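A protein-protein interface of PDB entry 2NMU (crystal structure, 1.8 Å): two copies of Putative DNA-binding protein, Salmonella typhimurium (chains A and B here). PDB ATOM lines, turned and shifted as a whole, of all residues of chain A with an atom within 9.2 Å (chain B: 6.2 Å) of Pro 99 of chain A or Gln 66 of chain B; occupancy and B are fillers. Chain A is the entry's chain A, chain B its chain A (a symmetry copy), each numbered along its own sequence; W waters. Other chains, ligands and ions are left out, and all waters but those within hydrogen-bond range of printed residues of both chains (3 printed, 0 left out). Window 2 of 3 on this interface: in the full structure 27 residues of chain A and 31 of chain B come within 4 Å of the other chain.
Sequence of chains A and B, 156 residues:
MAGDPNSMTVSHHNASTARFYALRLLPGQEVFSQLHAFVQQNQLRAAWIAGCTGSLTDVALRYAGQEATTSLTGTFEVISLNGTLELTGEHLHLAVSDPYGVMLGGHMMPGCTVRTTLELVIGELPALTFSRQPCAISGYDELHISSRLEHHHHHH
Of the 15 printed residues of chain A, 7 touch a printed residue of chain B. Hydrophobic or aromatic side chains of chain A within 4 Å of the printed part of chain B: Pro 99. Among the printed residues, no Asp or Glu carboxylate lies within 4 Å of a Lys or Arg side-chain nitrogen of the other chain.
No position is printed for both chains.
Water W1 lies within hydrogen-bond range of OG of Ser 97 of chain A (2.6 Å), O of Asp 98 of chain A (2.7 Å) and N of Ala 64 of chain B (3.0 Å). Water W2 lies within hydrogen-bond range of the side-chain carboxylate of Glu 77 of chain A (2.7 Å), the backbone NH of Gly 65 of chain B (3.0 Å) and the guanidinium group of Arg 115 of chain A (3.1 Å). Water W3 lies within hydrogen-bond range of O of Pro 99 of chain A and OE1 of Gln 66 of chain B.
Of chain B, only Tyr 63, Ala 64 and Gln 66 come within 4 Å of Pro 99 of chain A. Printed residues of chain B within 4 Å of Thr 75 of chain A: Ala 64 and Gly 65. Of the printed residues of chain A, Tyr 63 of chain B touches Asp 98, Pro 99, Tyr 100 and Gly 101. Gly 74 of chain A touches none of the printed residues of chain B. Leu 56 of chain A touches none of the printed residues of chain B. The nearest printed residue of chain B that does not touch Tyr 100 of chain A is Gln 66 of chain B (4.01 Å).
Ala 64 of chain B touches Thr 75 of chain A (CB to O, 3.3 Å). N of Gly 65 of chain B touches CG2 of Thr 75 of chain A, at 3.7 Å. Glu 77 of chain A touches Ala 64 of chain B (CG to CB, 3.5 Å). Ser 97 of chain A touches Ala 64 of chain B. O of Asp 98 of chain A touches CB of Tyr 63 of chain B (3.9 Å). Asp 98 of chain A touches Ala 64 of chain B. Pro 99 of chain A touches Tyr 63 of chain B. CB of Pro 99 of chain A touches O of Ala 64 of chain B, 3.2 Å away. CD2 of Tyr 63 of chain B touches C of Tyr 100 of chain A, at 3.8 Å. Tyr 63 of chain B touches Gly 101 of chain A.
N of Gly 101 of chain A sits at hydrogen-bond distance from OD1 of Asp 98 of chain A (3.3 Å). OE2 of Glu 77 of chain A is in salt-bridge range of NH2 of Arg 115 of chain A, 2.7 Å away. The side-chain carboxylate (OD1) of Asp 98 of chain A sits at hydrogen-bond distance from the backbone NH (N) of Tyr 100 of chain A, at 2.8 Å. The backbone NH (N) of Glu 77 of chain A is in hydrogen-bond range of the backbone carbonyl oxygen (O) of Ser 97 of chain A (3.0 Å). The side-chain carboxylate of Asp 98 of chain A is in hydrogen-bond range of the backbone NH of Val 102 of chain A.
The backbone carbonyl oxygen of Pro 99 of chain A lies close to the side-chain amide oxygen of Gln 66 of chain B (2.9 Å).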
ATOM      1  N   LEU A  56      30.393   3.640   2.423  1.00  0.00           N
ATOM      2  CA  LEU A  56      31.736   4.117   2.721  1.00  0.00           C
ATOM      3  C   LEU A  56      32.174   5.202   1.744  1.00  0.00           C
ATOM      4  O   LEU A  56      31.655   5.304   0.629  1.00  0.00           O
ATOM      5  CB  LEU A  56      32.743   2.964   2.639  1.00  0.00           C
ATOM      6  CG  LEU A  56      32.526   1.730   3.519  1.00  0.00           C
ATOM      7  CD1 LEU A  56      33.475   0.628   3.082  1.00  0.00           C
ATOM      8  CD2 LEU A  56      32.747   2.089   4.981  1.00  0.00           C
ATOM      9  N   THR A  73      38.696   6.300  -2.899  1.00  0.00           N
ATOM     10  CA  THR A  73      37.847   7.316  -2.299  1.00  0.00           C
ATOM     11  C   THR A  73      36.726   7.584  -3.292  1.00  0.00           C
ATOM     12  O   THR A  73      36.973   7.729  -4.489  1.00  0.00           O
ATOM     13  CB  THR A  73      38.614   8.636  -2.032  1.00  0.00           C
ATOM     14  OG1 THR A  73      39.647   8.409  -1.065  1.00  0.00           O
ATOM     15  CG2 THR A  73      37.666   9.704  -1.499  1.00  0.00           C
ATOM     16  N   GLY A  74      35.496   7.633  -2.797  1.00  0.00           N
ATOM     17  CA  GLY A  74      34.365   7.880  -3.671  1.00  0.00           C
ATOM     18  C   GLY A  74      33.052   7.680  -2.945  1.00  0.00           C
ATOM     19  O   GLY A  74      32.929   7.997  -1.763  1.00  0.00           O
ATOM     20  N   THR A  75      32.069   7.154  -3.663  1.00  0.00           N
ATOM     21  CA  THR A  75      30.747   6.898  -3.107  1.00  0.00           C
ATOM     22  C   THR A  75      30.521   5.402  -3.248  1.00  0.00           C
ATOM     23  O   THR A  75      30.265   4.908  -4.344  1.00  0.00           O
ATOM     24  CB  THR A  75      29.667   7.665  -3.893  1.00  0.00           C
ATOM     25  OG1 THR A  75      29.984   9.062  -3.877  1.00  0.00           O
ATOM     26  CG2 THR A  75      28.292   7.459  -3.267  1.00  0.00           C
ATOM     27  N   PHE A  76      30.615   4.687  -2.134  1.00  0.00           N
ATOM     28  CA  PHE A  76      30.478   3.235  -2.142  1.00  0.00           C
ATOM     29  C   PHE A  76      29.423   2.685  -1.191  1.00  0.00           C
ATOM     30  O   PHE A  76      29.169   3.249  -0.126  1.00  0.00           O
ATOM     31  CB  PHE A  76      31.813   2.593  -1.756  1.00  0.00           C
ATOM     32  CG  PHE A  76      32.937   2.878  -2.707  1.00  0.00           C
ATOM     33  CD1 PHE A  76      33.064   2.164  -3.890  1.00  0.00           C
ATOM     34  CD2 PHE A  76      33.896   3.842  -2.403  1.00  0.00           C
ATOM     35  CE1 PHE A  76      34.132   2.399  -4.757  1.00  0.00           C
ATOM     36  CE2 PHE A  76      34.967   4.085  -3.263  1.00  0.00           C
ATOM     37  CZ  PHE A  76      35.085   3.361  -4.442  1.00  0.00           C
ATOM     38  N   GLU A  77      28.812   1.575  -1.587  1.00  0.00           N
ATOM     39  CA  GLU A  77      27.837   0.894  -0.747  1.00  0.00           C
ATOM     40  C   GLU A  77      28.550  -0.372  -0.294  1.00  0.00           C
ATOM     41  O   GLU A  77      29.284  -0.984  -1.073  1.00  0.00           O
ATOM     42  CB  GLU A  77      26.588   0.493  -1.542  1.00  0.00           C
ATOM     43  CG  GLU A  77      25.698   1.647  -1.974  1.00  0.00           C
ATOM     44  CD  GLU A  77      24.994   2.305  -0.808  1.00  0.00           C
ATOM     45  OE1 GLU A  77      24.065   1.691  -0.241  1.00  0.00           O
ATOM     46  OE2 GLU A  77      25.372   3.438  -0.450  1.00  0.00           O
ATOM     47  N   VAL A  96      32.438  -3.877  -2.116  1.00  0.00           N
ATOM     48  CA  VAL A  96      31.707  -2.620  -2.253  1.00  0.00           C
ATOM     49  C   VAL A  96      31.253  -2.421  -3.692  1.00  0.00           C
ATOM     50  O   VAL A  96      31.832  -2.997  -4.611  1.00  0.00           O
ATOM     51  CB  VAL A  96      32.571  -1.398  -1.846  1.00  0.00           C
ATOM     52  CG1 VAL A  96      32.914  -1.467  -0.367  1.00  0.00           C
ATOM     53  CG2 VAL A  96      33.839  -1.347  -2.684  1.00  0.00           C
ATOM     54  N   SER A  97      30.209  -1.613  -3.874  1.00  0.00           N
ATOM     55  CA  SER A  97      29.673  -1.305  -5.200  1.00  0.00           C
ATOM     56  C   SER A  97      29.675   0.211  -5.369  1.00  0.00           C
ATOM     57  O   SER A  97      29.428   0.942  -4.405  1.00  0.00           O
ATOM     58  CB  SER A  97      28.245  -1.851  -5.353  1.00  0.00           C
ATOM     59  OG  SER A  97      27.342  -1.270  -4.424  1.00  0.00           O
ATOM     60  N   ASP A  98      29.963   0.684  -6.582  1.00  0.00           N
ATOM     61  CA  ASP A  98      30.004   2.124  -6.836  1.00  0.00           C
ATOM     62  C   ASP A  98      28.696   2.660  -7.438  1.00  0.00           C
ATOM     63  O   ASP A  98      27.727   1.911  -7.601  1.00  0.00           O
ATOM     64  CB  ASP A  98      31.213   2.485  -7.720  1.00  0.00           C
ATOM     65  CG  ASP A  98      31.106   1.949  -9.137  1.00  0.00           C
ATOM     66  OD1 ASP A  98      29.994   1.600  -9.574  1.00  0.00           O
ATOM     67  OD2 ASP A  98      32.154   1.904  -9.821  1.00  0.00           O
ATOM     68  N   PRO A  99      28.642   3.965  -7.769  1.00  0.00           N
ATOM     69  CA  PRO A  99      27.420   4.546  -8.334  1.00  0.00           C
ATOM     70  C   PRO A  99      26.914   3.943  -9.639  1.00  0.00           C
ATOM     71  O   PRO A  99      25.843   4.314 -10.118  1.00  0.00           O
ATOM     72  CB  PRO A  99      27.780   6.025  -8.490  1.00  0.00           C
ATOM     73  CG  PRO A  99      28.785   6.250  -7.415  1.00  0.00           C
ATOM     74  CD  PRO A  99      29.648   5.016  -7.540  1.00  0.00           C
ATOM     75  N   TYR A 100      27.670   3.015 -10.209  1.00  0.00           N
ATOM     76  CA  TYR A 100      27.265   2.406 -11.467  1.00  0.00           C
ATOM     77  C   TYR A 100      27.095   0.890 -11.357  1.00  0.00           C
ATOM     78  O   TYR A 100      27.019   0.181 -12.364  1.00  0.00           O
ATOM     79  CB  TYR A 100      28.277   2.794 -12.545  1.00  0.00           C
ATOM     80  CG  TYR A 100      28.452   4.293 -12.592  1.00  0.00           C
ATOM     81  CD1 TYR A 100      27.418   5.119 -13.026  1.00  0.00           C
ATOM     82  CD2 TYR A 100      29.606   4.896 -12.098  1.00  0.00           C
ATOM     83  CE1 TYR A 100      27.523   6.514 -12.958  1.00  0.00           C
ATOM     84  CE2 TYR A 100      29.723   6.291 -12.024  1.00  0.00           C
ATOM     85  CZ  TYR A 100      28.677   7.090 -12.451  1.00  0.00           C
ATOM     86  OH  TYR A 100      28.771   8.461 -12.351  1.00  0.00           O
ATOM     87  N   GLY A 101      27.019   0.408 -10.119  1.00  0.00           N
ATOM     88  CA  GLY A 101      26.821  -1.010  -9.869  1.00  0.00           C
ATOM     89  C   GLY A 101      28.067  -1.872  -9.861  1.00  0.00           C
ATOM     90  O   GLY A 101      28.010  -3.038  -9.458  1.00  0.00           O
ATOM     91  N   VAL A 102      29.187  -1.305 -10.300  1.00  0.00           N
ATOM     92  CA  VAL A 102      30.452  -2.028 -10.356  1.00  0.00           C
ATOM     93  C   VAL A 102      30.964  -2.385  -8.967  1.00  0.00           C
ATOM     94  O   VAL A 102      30.989  -1.545  -8.066  1.00  0.00           O
ATOM     95  CB  VAL A 102      31.524  -1.193 -11.073  1.00  0.00           C
ATOM     96  CG1 VAL A 102      32.801  -2.005 -11.223  1.00  0.00           C
ATOM     97  CG2 VAL A 102      31.000  -0.744 -12.436  1.00  0.00           C
ATOM     98  N   MET A 103      31.392  -3.631  -8.800  1.00  0.00           N
ATOM     99  CA  MET A 103      31.878  -4.080  -7.505  1.00  0.00           C
ATOM    100  C   MET A 103      33.376  -4.367  -7.466  1.00  0.00           C
ATOM    101  O   MET A 103      33.991  -4.709  -8.475  1.00  0.00           O
ATOM    102  CB  MET A 103      31.084  -5.317  -7.066  1.00  0.00           C
ATOM    103  CG  MET A 103      29.639  -5.015  -6.672  1.00  0.00           C
ATOM    104  SD  MET A 103      28.604  -6.591  -6.244  1.00  0.00           S
ATOM    105  CE  MET A 103      29.511  -7.086  -4.602  1.00  0.00           C
ATOM    106  N   ARG A 115      30.401   6.444   5.285  1.00  0.00           N
ATOM    107  CA  ARG A 115      29.848   7.578   4.552  1.00  0.00           C
ATOM    108  C   ARG A 115      28.603   8.077   5.281  1.00  0.00           C
ATOM    109  O   ARG A 115      28.626   9.154   5.873  1.00  0.00           O
ATOM    110  CB  ARG A 115      29.508   7.177   3.112  1.00  0.00           C
ATOM    111  CG  ARG A 115      29.040   8.336   2.233  1.00  0.00           C
ATOM    112  CD  ARG A 115      29.364   8.079   0.764  1.00  0.00           C
ATOM    113  NE  ARG A 115      28.750   6.853   0.264  1.00  0.00           N
ATOM    114  CZ  ARG A 115      27.454   6.717  -0.003  1.00  0.00           C
ATOM    115  NH1 ARG A 115      26.625   7.740   0.179  1.00  0.00           N
ATOM    116  NH2 ARG A 115      26.985   5.558  -0.446  1.00  0.00           N
ATOM    117  N   ARG B  62      19.350   0.303  -6.215  1.00  0.00           N
ATOM    118  CA  ARG B  62      19.614   1.729  -6.211  1.00  0.00           C
ATOM    119  C   ARG B  62      21.116   1.793  -5.974  1.00  0.00           C
ATOM    120  O   ARG B  62      21.598   1.455  -4.890  1.00  0.00           O
ATOM    121  CB  ARG B  62      18.863   2.427  -5.080  1.00  0.00           C
ATOM    122  CG  ARG B  62      18.836   3.941  -5.217  1.00  0.00           C
ATOM    123  CD  ARG B  62      18.084   4.574  -4.067  1.00  0.00           C
ATOM    124  NE  ARG B  62      18.781   4.366  -2.804  1.00  0.00           N
ATOM    125  CZ  ARG B  62      18.290   4.696  -1.614  1.00  0.00           C
ATOM    126  NH1 ARG B  62      17.085   5.252  -1.522  1.00  0.00           N
ATOM    127  NH2 ARG B  62      19.001   4.471  -0.517  1.00  0.00           N
ATOM    128  N   TYR B  63      21.863   2.196  -6.995  1.00  0.00           N
ATOM    129  CA  TYR B  63      23.310   2.258  -6.869  1.00  0.00           C
ATOM    130  C   TYR B  63      23.777   3.354  -5.919  1.00  0.00           C
ATOM    131  O   TYR B  63      23.041   4.294  -5.623  1.00  0.00           O
ATOM    132  CB  TYR B  63      23.955   2.438  -8.242  1.00  0.00           C
ATOM    133  CG  TYR B  63      23.664   1.304  -9.201  1.00  0.00           C
ATOM    134  CD1 TYR B  63      23.629  -0.019  -8.764  1.00  0.00           C
ATOM    135  CD2 TYR B  63      23.462   1.551 -10.553  1.00  0.00           C
ATOM    136  CE1 TYR B  63      23.400  -1.071  -9.658  1.00  0.00           C
ATOM    137  CE2 TYR B  63      23.236   0.511 -11.452  1.00  0.00           C
ATOM    138  CZ  TYR B  63      23.208  -0.793 -10.999  1.00  0.00           C
ATOM    139  OH  TYR B  63      23.003  -1.814 -11.899  1.00  0.00           O
ATOM    140  N   ALA B  64      25.013   3.218  -5.443  1.00  0.00           N
ATOM    141  CA  ALA B  64      25.603   4.165  -4.503  1.00  0.00           C
ATOM    142  C   ALA B  64      25.424   5.631  -4.886  1.00  0.00           C
ATOM    143  O   ALA B  64      25.798   6.045  -5.982  1.00  0.00           O
ATOM    144  CB  ALA B  64      27.090   3.858  -4.325  1.00  0.00           C
ATOM    145  N   GLY B  65      24.848   6.403  -3.969  1.00  0.00           N
ATOM    146  CA  GLY B  65      24.647   7.825  -4.196  1.00  0.00           C
ATOM    147  C   GLY B  65      23.591   8.204  -5.218  1.00  0.00           C
ATOM    148  O   GLY B  65      23.348   9.389  -5.445  1.00  0.00           O
ATOM    149  N   GLN B  66      22.961   7.212  -5.837  1.00  0.00           N
ATOM    150  CA  GLN B  66      21.935   7.476  -6.836  1.00  0.00           C
ATOM    151  C   GLN B  66      20.572   7.661  -6.169  1.00  0.00           C
ATOM    152  O   GLN B  66      20.304   7.093  -5.111  1.00  0.00           O
ATOM    153  CB  GLN B  66      21.865   6.321  -7.840  1.00  0.00           C
ATOM    154  CG  GLN B  66      23.178   6.012  -8.549  1.00  0.00           C
ATOM    155  CD  GLN B  66      23.563   7.052  -9.588  1.00  0.00           C
ATOM    156  OE1 GLN B  66      24.596   6.930 -10.251  1.00  0.00           O
ATOM    157  NE2 GLN B  66      22.734   8.077  -9.739  1.00  0.00           N
ATOM    158  N   GLU B  67      19.716   8.460  -6.796  1.00  0.00           N
ATOM    159  CA  GLU B  67      18.382   8.718  -6.271  1.00  0.00           C
ATOM    160  C   GLU B  67      17.378   7.795  -6.949  1.00  0.00           C
ATOM    161  O   GLU B  67      16.418   7.338  -6.329  1.00  0.00           O
ATOM    162  CB  GLU B  67      17.995  10.178  -6.524  1.00  0.00           C
ATOM    163  CG  GLU B  67      16.547  10.523  -6.196  1.00  0.00           C
ATOM    164  CD  GLU B  67      16.230  10.414  -4.716  1.00  0.00           C
ATOM    165  OE1 GLU B  67      16.352   9.303  -4.156  1.00  0.00           O
ATOM    166  OE2 GLU B  67      15.859  11.444  -4.112  1.00  0.00           O
ATOM    167  N   ALA B  68      17.614   7.517  -8.227  1.00  0.00           N
ATOM    168  CA  ALA B  68      16.727   6.662  -8.999  1.00  0.00           C
ATOM    169  C   ALA B  68      17.070   5.190  -8.865  1.00  0.00           C
ATOM    170  O   ALA B  68      18.214   4.823  -8.606  1.00  0.00           O
ATOM    171  CB  ALA B  68      16.768   7.062 -10.462  1.00  0.00           C
HETATM  172  O   HOH W   1      26.095   0.455  -5.987  1.00  0.00           O
HETATM  173  O   HOH W   2      23.952   5.595  -1.186  1.00  0.00           O
HETATM  174  O   HOH W   3      24.204   4.455 -12.596  1.00  0.00           O
